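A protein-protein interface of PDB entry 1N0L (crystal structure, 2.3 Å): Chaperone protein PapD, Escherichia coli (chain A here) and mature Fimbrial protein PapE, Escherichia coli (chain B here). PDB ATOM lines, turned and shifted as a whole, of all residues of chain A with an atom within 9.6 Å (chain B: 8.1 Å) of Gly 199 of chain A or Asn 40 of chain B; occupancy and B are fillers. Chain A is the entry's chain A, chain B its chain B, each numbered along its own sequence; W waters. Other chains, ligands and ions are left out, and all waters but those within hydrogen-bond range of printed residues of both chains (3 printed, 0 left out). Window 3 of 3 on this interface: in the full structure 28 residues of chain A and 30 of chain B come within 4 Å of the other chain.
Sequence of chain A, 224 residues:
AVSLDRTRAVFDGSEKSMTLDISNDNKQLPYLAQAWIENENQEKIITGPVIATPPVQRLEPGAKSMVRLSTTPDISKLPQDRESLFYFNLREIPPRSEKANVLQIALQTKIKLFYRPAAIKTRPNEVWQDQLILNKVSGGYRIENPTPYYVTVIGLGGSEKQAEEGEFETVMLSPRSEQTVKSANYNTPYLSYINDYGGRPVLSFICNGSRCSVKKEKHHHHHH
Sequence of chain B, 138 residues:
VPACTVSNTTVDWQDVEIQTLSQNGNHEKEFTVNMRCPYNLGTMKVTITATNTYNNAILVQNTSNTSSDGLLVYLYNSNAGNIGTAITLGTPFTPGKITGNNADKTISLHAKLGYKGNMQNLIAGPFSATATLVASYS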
ATOM      1  N   THR A   7     -19.341   6.860  27.611  1.00  0.00           N
ATOM      2  CA  THR A   7     -20.101   7.342  28.763  1.00  0.00           C
ATOM      3  C   THR A   7     -21.598   7.126  28.605  1.00  0.00           C
ATOM      4  O   THR A   7     -22.371   7.447  29.495  1.00  0.00           O
ATOM      5  CB  THR A   7     -19.829   8.827  29.035  1.00  0.00           C
ATOM      6  OG1 THR A   7     -20.186   9.599  27.882  1.00  0.00           O
ATOM      7  CG2 THR A   7     -18.352   9.035  29.351  1.00  0.00           C
ATOM      8  N   ARG A   8     -21.989   6.590  27.454  1.00  0.00           N
ATOM      9  CA  ARG A   8     -23.381   6.245  27.167  1.00  0.00           C
ATOM     10  C   ARG A   8     -23.310   5.290  25.992  1.00  0.00           C
ATOM     11  O   ARG A   8     -22.325   5.275  25.259  1.00  0.00           O
ATOM     12  CB  ARG A   8     -24.212   7.467  26.776  1.00  0.00           C
ATOM     13  CG  ARG A   8     -23.830   8.107  25.449  1.00  0.00           C
ATOM     14  CD  ARG A   8     -24.081   9.586  25.552  1.00  0.00           C
ATOM     15  NE  ARG A   8     -23.397  10.040  26.745  1.00  0.00           N
ATOM     16  CZ  ARG A   8     -23.913  10.840  27.668  1.00  0.00           C
ATOM     17  NH1 ARG A   8     -25.152  11.313  27.550  1.00  0.00           N
ATOM     18  NH2 ARG A   8     -23.182  11.121  28.740  1.00  0.00           N
ATOM     19  N   GLN A 129     -31.590  17.754  18.970  1.00  0.00           N
ATOM     20  CA  GLN A 129     -31.718  18.533  20.193  1.00  0.00           C
ATOM     21  C   GLN A 129     -32.003  19.997  19.965  1.00  0.00           C
ATOM     22  O   GLN A 129     -32.383  20.712  20.894  1.00  0.00           O
ATOM     23  CB  GLN A 129     -30.474  18.375  21.070  1.00  0.00           C
ATOM     24  CG  GLN A 129     -30.218  16.942  21.490  1.00  0.00           C
ATOM     25  CD  GLN A 129     -29.270  16.224  20.551  1.00  0.00           C
ATOM     26  OE1 GLN A 129     -29.126  16.600  19.380  1.00  0.00           O
ATOM     27  NE2 GLN A 129     -28.622  15.181  21.057  1.00  0.00           N
ATOM     28  N   THR A 152     -30.431  14.937  27.312  1.00  0.00           N
ATOM     29  CA  THR A 152     -29.815  15.315  28.566  1.00  0.00           C
ATOM     30  C   THR A 152     -29.262  16.717  28.450  1.00  0.00           C
ATOM     31  O   THR A 152     -28.410  16.992  27.604  1.00  0.00           O
ATOM     32  CB  THR A 152     -28.683  14.348  28.936  1.00  0.00           C
ATOM     33  OG1 THR A 152     -29.187  13.007  28.910  1.00  0.00           O
ATOM     34  CG2 THR A 152     -28.142  14.678  30.339  1.00  0.00           C
ATOM     35  N   ILE A 154     -27.277  19.759  30.294  1.00  0.00           N
ATOM     36  CA  ILE A 154     -26.313  19.993  31.359  1.00  0.00           C
ATOM     37  C   ILE A 154     -26.032  21.460  31.632  1.00  0.00           C
ATOM     38  O   ILE A 154     -25.354  21.794  32.601  1.00  0.00           O
ATOM     39  CB  ILE A 154     -24.986  19.300  31.043  1.00  0.00           C
ATOM     40  CG1 ILE A 154     -24.432  19.848  29.724  1.00  0.00           C
ATOM     41  CG2 ILE A 154     -25.202  17.795  30.967  1.00  0.00           C
ATOM     42  CD1 ILE A 154     -23.007  19.451  29.444  1.00  0.00           C
ATOM     43  N   GLU A 164     -22.016  26.727  29.476  1.00  0.00           N
ATOM     44  CA  GLU A 164     -20.986  25.697  29.531  1.00  0.00           C
ATOM     45  C   GLU A 164     -20.484  25.496  30.958  1.00  0.00           C
ATOM     46  O   GLU A 164     -20.332  24.371  31.426  1.00  0.00           O
ATOM     47  CB  GLU A 164     -19.826  26.057  28.599  1.00  0.00           C
ATOM     48  CG  GLU A 164     -20.253  26.281  27.156  1.00  0.00           C
ATOM     49  CD  GLU A 164     -19.086  26.289  26.194  1.00  0.00           C
ATOM     50  OE1 GLU A 164     -18.581  25.197  25.854  1.00  0.00           O
ATOM     51  OE2 GLU A 164     -18.663  27.392  25.784  1.00  0.00           O
ATOM     52  N   GLU A 165     -20.227  26.597  31.646  1.00  0.00           N
ATOM     53  CA  GLU A 165     -19.770  26.545  33.023  1.00  0.00           C
ATOM     54  C   GLU A 165     -20.728  27.419  33.825  1.00  0.00           C
ATOM     55  O   GLU A 165     -20.843  28.620  33.580  1.00  0.00           O
ATOM     56  CB  GLU A 165     -18.334  27.070  33.123  1.00  0.00           C
ATOM     57  CG  GLU A 165     -18.112  28.416  32.441  1.00  0.00           C
ATOM     58  CD  GLU A 165     -16.663  28.878  32.492  1.00  0.00           C
ATOM     59  OE1 GLU A 165     -16.157  29.129  33.607  1.00  0.00           O
ATOM     60  OE2 GLU A 165     -16.032  28.988  31.417  1.00  0.00           O
ATOM     61  N   SER A 192     -26.929  23.791  26.871  1.00  0.00           N
ATOM     62  CA  SER A 192     -25.902  22.830  26.504  1.00  0.00           C
ATOM     63  C   SER A 192     -26.432  21.441  26.804  1.00  0.00           C
ATOM     64  O   SER A 192     -27.120  21.236  27.801  1.00  0.00           O
ATOM     65  CB  SER A 192     -24.615  23.082  27.278  1.00  0.00           C
ATOM     66  OG  SER A 192     -23.544  22.397  26.650  1.00  0.00           O
ATOM     67  N   TYR A 193     -26.130  20.494  25.926  1.00  0.00           N
ATOM     68  CA  TYR A 193     -26.581  19.117  26.097  1.00  0.00           C
ATOM     69  C   TYR A 193     -25.453  18.144  25.703  1.00  0.00           C
ATOM     70  O   TYR A 193     -24.379  18.558  25.252  1.00  0.00           O
ATOM     71  CB  TYR A 193     -27.819  18.874  25.226  1.00  0.00           C
ATOM     72  CG  TYR A 193     -27.510  18.909  23.757  1.00  0.00           C
ATOM     73  CD1 TYR A 193     -27.216  17.733  23.055  1.00  0.00           C
ATOM     74  CD2 TYR A 193     -27.433  20.121  23.072  1.00  0.00           C
ATOM     75  CE1 TYR A 193     -26.852  17.768  21.703  1.00  0.00           C
ATOM     76  CE2 TYR A 193     -27.065  20.168  21.714  1.00  0.00           C
ATOM     77  CZ  TYR A 193     -26.778  18.989  21.038  1.00  0.00           C
ATOM     78  OH  TYR A 193     -26.431  19.029  19.700  1.00  0.00           O
ATOM     79  N   ILE A 194     -25.717  16.855  25.860  1.00  0.00           N
ATOM     80  CA  ILE A 194     -24.745  15.827  25.537  1.00  0.00           C
ATOM     81  C   ILE A 194     -25.211  14.951  24.379  1.00  0.00           C
ATOM     82  O   ILE A 194     -26.260  14.326  24.463  1.00  0.00           O
ATOM     83  CB  ILE A 194     -24.493  14.938  26.775  1.00  0.00           C
ATOM     84  CG1 ILE A 194     -24.103  15.834  27.964  1.00  0.00           C
ATOM     85  CG2 ILE A 194     -23.411  13.894  26.476  1.00  0.00           C
ATOM     86  CD1 ILE A 194     -23.902  15.095  29.292  1.00  0.00           C
ATOM     87  N   ASN A 195     -24.437  14.904  23.296  1.00  0.00           N
ATOM     88  CA  ASN A 195     -24.805  14.072  22.157  1.00  0.00           C
ATOM     89  C   ASN A 195     -24.430  12.607  22.388  1.00  0.00           C
ATOM     90  O   ASN A 195     -23.828  12.259  23.402  1.00  0.00           O
ATOM     91  CB  ASN A 195     -24.158  14.581  20.850  1.00  0.00           C
ATOM     92  CG  ASN A 195     -22.625  14.599  20.905  1.00  0.00           C
ATOM     93  OD1 ASN A 195     -22.010  13.838  21.640  1.00  0.00           O
ATOM     94  ND2 ASN A 195     -22.018  15.464  20.107  1.00  0.00           N
ATOM     95  N   ASP A 196     -24.803  11.759  21.435  1.00  0.00           N
ATOM     96  CA  ASP A 196     -24.542  10.326  21.490  1.00  0.00           C
ATOM     97  C   ASP A 196     -23.124   9.910  21.860  1.00  0.00           C
ATOM     98  O   ASP A 196     -22.936   8.880  22.504  1.00  0.00           O
ATOM     99  CB  ASP A 196     -24.883   9.684  20.140  1.00  0.00           C
ATOM    100  CG  ASP A 196     -26.379   9.577  19.900  1.00  0.00           C
ATOM    101  OD1 ASP A 196     -27.171  10.104  20.718  1.00  0.00           O
ATOM    102  OD2 ASP A 196     -26.755   8.963  18.884  1.00  0.00           O
ATOM    103  N   TYR A 197     -22.124  10.682  21.443  1.00  0.00           N
ATOM    104  CA  TYR A 197     -20.752  10.310  21.755  1.00  0.00           C
ATOM    105  C   TYR A 197     -20.067  11.131  22.839  1.00  0.00           C
ATOM    106  O   TYR A 197     -18.839  11.171  22.918  1.00  0.00           O
ATOM    107  CB  TYR A 197     -19.901  10.267  20.476  1.00  0.00           C
ATOM    108  CG  TYR A 197     -20.016  11.476  19.588  1.00  0.00           C
ATOM    109  CD1 TYR A 197     -19.218  12.601  19.803  1.00  0.00           C
ATOM    110  CD2 TYR A 197     -20.947  11.510  18.551  1.00  0.00           C
ATOM    111  CE1 TYR A 197     -19.351  13.746  18.997  1.00  0.00           C
ATOM    112  CE2 TYR A 197     -21.089  12.638  17.747  1.00  0.00           C
ATOM    113  CZ  TYR A 197     -20.291  13.755  17.975  1.00  0.00           C
ATOM    114  OH  TYR A 197     -20.452  14.892  17.208  1.00  0.00           O
ATOM    115  N   GLY A 198     -20.866  11.775  23.687  1.00  0.00           N
ATOM    116  CA  GLY A 198     -20.303  12.520  24.799  1.00  0.00           C
ATOM    117  C   GLY A 198     -19.846  13.937  24.567  1.00  0.00           C
ATOM    118  O   GLY A 198     -19.368  14.582  25.493  1.00  0.00           O
ATOM    119  N   GLY A 199     -19.957  14.412  23.334  1.00  0.00           N
ATOM    120  CA  GLY A 199     -19.589  15.782  23.047  1.00  0.00           C
ATOM    121  C   GLY A 199     -20.632  16.640  23.747  1.00  0.00           C
ATOM    122  O   GLY A 199     -21.742  16.154  24.010  1.00  0.00           O
ATOM    123  N   ARG A 200     -20.291  17.895  24.040  1.00  0.00           N
ATOM    124  CA  ARG A 200     -21.202  18.810  24.736  1.00  0.00           C
ATOM    125  C   ARG A 200     -21.434  20.123  23.991  1.00  0.00           C
ATOM    126  O   ARG A 200     -20.841  21.145  24.313  1.00  0.00           O
ATOM    127  CB  ARG A 200     -20.672  19.091  26.143  1.00  0.00           C
ATOM    128  CG  ARG A 200     -20.661  17.829  27.005  1.00  0.00           C
ATOM    129  CD  ARG A 200     -20.295  18.091  28.463  1.00  0.00           C
ATOM    130  NE  ARG A 200     -20.364  16.871  29.266  1.00  0.00           N
ATOM    131  CZ  ARG A 200     -20.483  16.851  30.591  1.00  0.00           C
ATOM    132  NH1 ARG A 200     -20.548  17.987  31.267  1.00  0.00           N
ATOM    133  NH2 ARG A 200     -20.532  15.693  31.242  1.00  0.00           N
ATOM    134  N   PRO A 201     -22.315  20.102  22.984  1.00  0.00           N
ATOM    135  CA  PRO A 201     -22.671  21.255  22.151  1.00  0.00           C
ATOM    136  C   PRO A 201     -23.517  22.295  22.879  1.00  0.00           C
ATOM    137  O   PRO A 201     -24.275  21.964  23.797  1.00  0.00           O
ATOM    138  CB  PRO A 201     -23.446  20.629  20.987  1.00  0.00           C
ATOM    139  CG  PRO A 201     -23.045  19.169  21.016  1.00  0.00           C
ATOM    140  CD  PRO A 201     -22.977  18.886  22.489  1.00  0.00           C
ATOM    141  N   VAL A 202     -23.380  23.546  22.454  1.00  0.00           N
ATOM    142  CA  VAL A 202     -24.140  24.642  23.035  1.00  0.00           C
ATOM    143  C   VAL A 202     -25.081  25.180  21.985  1.00  0.00           C
ATOM    144  O   VAL A 202     -24.670  25.485  20.864  1.00  0.00           O
ATOM    145  CB  VAL A 202     -23.244  25.813  23.481  1.00  0.00           C
ATOM    146  CG1 VAL A 202     -24.108  26.974  23.927  1.00  0.00           C
ATOM    147  CG2 VAL A 202     -22.340  25.377  24.589  1.00  0.00           C
ATOM    148  N   VAL B   1     -16.899   9.534  24.417  1.00  0.00           N
ATOM    149  CA  VAL B   1     -15.567   9.639  25.101  1.00  0.00           C
ATOM    150  C   VAL B   1     -15.441   8.556  26.172  1.00  0.00           C
ATOM    151  O   VAL B   1     -16.437   8.139  26.763  1.00  0.00           O
ATOM    152  CB  VAL B   1     -15.384  11.014  25.794  1.00  0.00           C
ATOM    153  CG1 VAL B   1     -13.901  11.293  25.998  1.00  0.00           C
ATOM    154  CG2 VAL B   1     -16.017  12.130  24.962  1.00  0.00           C
ATOM    155  N   PRO B   2     -14.210   8.082  26.432  1.00  0.00           N
ATOM    156  CA  PRO B   2     -14.000   7.044  27.447  1.00  0.00           C
ATOM    157  C   PRO B   2     -14.364   7.493  28.860  1.00  0.00           C
ATOM    158  O   PRO B   2     -14.167   8.653  29.228  1.00  0.00           O
ATOM    159  CB  PRO B   2     -12.511   6.710  27.305  1.00  0.00           C
ATOM    160  CG  PRO B   2     -11.922   7.995  26.763  1.00  0.00           C
ATOM    161  CD  PRO B   2     -12.946   8.406  25.744  1.00  0.00           C
ATOM    162  N   CYS B  37     -10.343  11.444  33.908  1.00  0.00           N
ATOM    163  CA  CYS B  37     -11.599  11.584  33.182  1.00  0.00           C
ATOM    164  C   CYS B  37     -11.607  12.232  31.793  1.00  0.00           C
ATOM    165  O   CYS B  37     -10.592  12.741  31.319  1.00  0.00           O
ATOM    166  CB  CYS B  37     -12.578  12.351  34.062  1.00  0.00           C
ATOM    167  SG  CYS B  37     -13.077  11.587  35.645  1.00  0.00           S
ATOM    168  N   PRO B  38     -12.776  12.188  31.117  1.00  0.00           N
ATOM    169  CA  PRO B  38     -13.000  12.761  29.790  1.00  0.00           C
ATOM    170  C   PRO B  38     -12.611  14.234  29.835  1.00  0.00           C
ATOM    171  O   PRO B  38     -12.746  14.878  30.873  1.00  0.00           O
ATOM    172  CB  PRO B  38     -14.503  12.598  29.601  1.00  0.00           C
ATOM    173  CG  PRO B  38     -14.787  11.340  30.276  1.00  0.00           C
ATOM    174  CD  PRO B  38     -13.938  11.378  31.527  1.00  0.00           C
ATOM    175  N   TYR B  39     -12.154  14.772  28.711  1.00  0.00           N
ATOM    176  CA  TYR B  39     -11.740  16.172  28.663  1.00  0.00           C
ATOM    177  C   TYR B  39     -12.858  17.155  28.990  1.00  0.00           C
ATOM    178  O   TYR B  39     -12.597  18.249  29.460  1.00  0.00           O
ATOM    179  CB  TYR B  39     -11.186  16.507  27.275  1.00  0.00           C
ATOM    180  CG  TYR B  39     -12.224  16.433  26.174  1.00  0.00           C
ATOM    181  CD1 TYR B  39     -12.945  17.565  25.780  1.00  0.00           C
ATOM    182  CD2 TYR B  39     -12.513  15.223  25.559  1.00  0.00           C
ATOM    183  CE1 TYR B  39     -13.936  17.481  24.799  1.00  0.00           C
ATOM    184  CE2 TYR B  39     -13.492  15.127  24.584  1.00  0.00           C
ATOM    185  CZ  TYR B  39     -14.201  16.256  24.210  1.00  0.00           C
ATOM    186  OH  TYR B  39     -15.173  16.134  23.249  1.00  0.00           O
ATOM    187  N   ASN B  40     -14.101  16.766  28.742  1.00  0.00           N
ATOM    188  CA  ASN B  40     -15.212  17.676  28.981  1.00  0.00           C
ATOM    189  C   ASN B  40     -16.161  17.319  30.122  1.00  0.00           C
ATOM    190  O   ASN B  40     -17.269  17.839  30.173  1.00  0.00           O
ATOM    191  CB  ASN B  40     -16.026  17.844  27.685  1.00  0.00           C
ATOM    192  CG  ASN B  40     -16.699  16.556  27.250  1.00  0.00           C
ATOM    193  OD1 ASN B  40     -16.685  15.557  27.977  1.00  0.00           O
ATOM    194  ND2 ASN B  40     -17.300  16.573  26.066  1.00  0.00           N
ATOM    195  N   LEU B  41     -15.752  16.440  31.030  1.00  0.00           N
ATOM    196  CA  LEU B  41     -16.631  16.079  32.138  1.00  0.00           C
ATOM    197  C   LEU B  41     -16.936  17.329  32.979  1.00  0.00           C
ATOM    198  O   LEU B  41     -16.046  18.140  33.260  1.00  0.00           O
ATOM    199  CB  LEU B  41     -15.983  15.003  33.010  1.00  0.00           C
ATOM    200  CG  LEU B  41     -16.990  14.164  33.805  1.00  0.00           C
ATOM    201  CD1 LEU B  41     -17.841  13.361  32.830  1.00  0.00           C
ATOM    202  CD2 LEU B  41     -16.269  13.222  34.758  1.00  0.00           C
ATOM    203  N   GLY B  42     -18.196  17.474  33.384  1.00  0.00           N
ATOM    204  CA  GLY B  42     -18.600  18.637  34.153  1.00  0.00           C
ATOM    205  C   GLY B  42     -18.446  18.616  35.664  1.00  0.00           C
ATOM    206  O   GLY B  42     -17.349  18.769  36.204  1.00  0.00           O
ATOM    207  N   THR B  43     -19.562  18.435  36.358  1.00  0.00           N
ATOM    208  CA  THR B  43     -19.551  18.434  37.816  1.00  0.00           C
ATOM    209  C   THR B  43     -19.922  17.089  38.414  1.00  0.00           C
ATOM    210  O   THR B  43     -19.788  16.890  39.615  1.00  0.00           O
ATOM    211  CB  THR B  43     -20.523  19.501  38.366  1.00  0.00           C
ATOM    212  OG1 THR B  43     -21.830  19.295  37.807  1.00  0.00           O
ATOM    213  CG2 THR B  43     -20.033  20.898  38.007  1.00  0.00           C
ATOM    214  N   ASN B 102      -9.463  17.370  34.552  1.00  0.00           N
ATOM    215  CA  ASN B 102     -10.257  16.184  34.265  1.00  0.00           C
ATOM    216  C   ASN B 102      -9.338  14.999  34.012  1.00  0.00           C
ATOM    217  O   ASN B 102      -9.529  13.920  34.571  1.00  0.00           O
ATOM    218  CB  ASN B 102     -11.144  16.412  33.038  1.00  0.00           C
ATOM    219  CG  ASN B 102     -12.484  17.029  33.390  1.00  0.00           C
ATOM    220  OD1 ASN B 102     -13.126  16.623  34.356  1.00  0.00           O
ATOM    221  ND2 ASN B 102     -12.920  18.002  32.595  1.00  0.00           N
ATOM    222  N   ALA B 103      -8.331  15.218  33.172  1.00  0.00           N
ATOM    223  CA  ALA B 103      -7.370  14.178  32.816  1.00  0.00           C
ATOM    224  C   ALA B 103      -6.639  13.578  34.013  1.00  0.00           C
ATOM    225  O   ALA B 103      -6.071  12.487  33.918  1.00  0.00           O
ATOM    226  CB  ALA B 103      -6.365  14.730  31.831  1.00  0.00           C
ATOM    227  N   LYS B 105      -7.777  14.006  37.937  1.00  0.00           N
ATOM    228  CA  LYS B 105      -8.466  14.514  39.120  1.00  0.00           C
ATOM    229  C   LYS B 105      -8.036  13.810  40.397  1.00  0.00           C
ATOM    230  O   LYS B 105      -7.264  12.850  40.368  1.00  0.00           O
ATOM    231  CB  LYS B 105      -9.983  14.380  38.966  1.00  0.00           C
ATOM    232  CG  LYS B 105     -10.614  15.420  38.068  1.00  0.00           C
ATOM    233  CD  LYS B 105     -12.133  15.324  38.097  1.00  0.00           C
ATOM    234  CE  LYS B 105     -12.769  16.459  37.308  1.00  0.00           C
ATOM    235  NZ  LYS B 105     -14.257  16.406  37.338  1.00  0.00           N
HETATM  236  O   HOH W   1     -19.666   9.004  25.499  1.00  0.00           O
HETATM  237  O   HOH W   2     -20.872  15.782  34.156  1.00  0.00           O
HETATM  238  O   HOH W   3     -19.071  14.327  28.180  1.00  0.00           O
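Of chain B, only Asn 40 comes within 4 Å of Gly 199 of chain A. Asn 40 of chain B touches just these residues of chain A: Gly 198 (2.9 Å), Gly 199 (3.9 Å) and Arg 200 (3.4 Å). No residue of chain A comes within 4 Å of Tyr 39 of chain B. Printed residues of chain B within 4 Å of Thr 7 of chain A: Val 1 (3.3 Å). Of the printed residues of chain B, Arg 200 of chain A touches Asn 40, Leu 41 and Gly 42. Of the printed residues of chain A, Gly 42 of chain B touches Arg 200 (3.2 Å). The nearest residue of chain B that does not touch Gly 199 of chain A is Tyr 39 of chain B (4.4 Å). The nearest residue of chain A that does not touch Asn 40 of chain B is Ile 154 of chain A (6.0 Å).
Among the printed residues, merely in contact across the chains: Gly 199 of chain A with Asn 40 of chain B (3.9 Å) and Arg 200 of chain A with Leu 41 of chain B (3.9 Å).
N of Thr 7 of chain A lies within hydrogen-bond range of O of Val 1 of chain B (3.3 Å). The backbone carbonyl oxygen (O) of Tyr 197 of chain A lies within hydrogen-bond range of the backbone NH (N) of Val 1 of chain B (2.9 Å). O of Gly 198 of chain A is in hydrogen-bond range of ND2 of Asn 40 of chain B (2.9 Å). NE of Arg 200 of chain A lies within hydrogen-bond range of O of Asn 40 of chain B. The guanidinium group (NH1) of Arg 200 of chain A sits close to the backbone NH (N) of Gly 42 of chain B.
Of the 18 printed residues of chain A, 5 touch a printed residue of chain B. Printed residues of chain B that touch a printed residue of chain A: Val 1, Asn 40, Leu 41 and Gly 42. Among the printed residues, 7 pairs touch across the chains. Among the printed residues, no Asp or Glu carboxylate lies within 4 Å of a Lys or Arg side-chain nitrogen of the other chain.
The side-chain hydroxyl (OG1) of Thr 7 of chain A is in hydrogen-bond range of the guanidinium group (NE) of Arg 8 of chain A (3.4 Å). N of Tyr 197 of chain A sits close to OD1 of Asn 195 of chain A, at 3.2 Å. The side-chain amide oxygen of Asn 195 of chain A is in hydrogen-bond range of the backbone NH of Gly 198 of chain A. The side-chain amide oxygen of Asn 195 of chain A sits at hydrogen-bond distance from the backbone NH of Gly 199 of chain A (2.7 Å). The side-chain amide nitrogen (ND2) of Asn 102 of chain B is in hydrogen-bond range of the backbone carbonyl oxygen (O) of Leu 41 of chain B (3.2 Å).
Water W1 lies within hydrogen-bond range of the side-chain hydroxyl (OG1) of Thr 7 of chain A, the backbone NH (N) of Val 1 of chain B and the backbone carbonyl oxygen (O) of Tyr 197 of chain A. Water W3 lies within hydrogen-bond range of OD1 of Asn 40 of chain B, O of Gly 198 of chain A and NE of Arg 200 of chain A. Water W2 lies within hydrogen-bond range of NH2 of Arg 200 of chain A (2.9 Å) and N of Gly 42 of chain B (3.3 Å).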
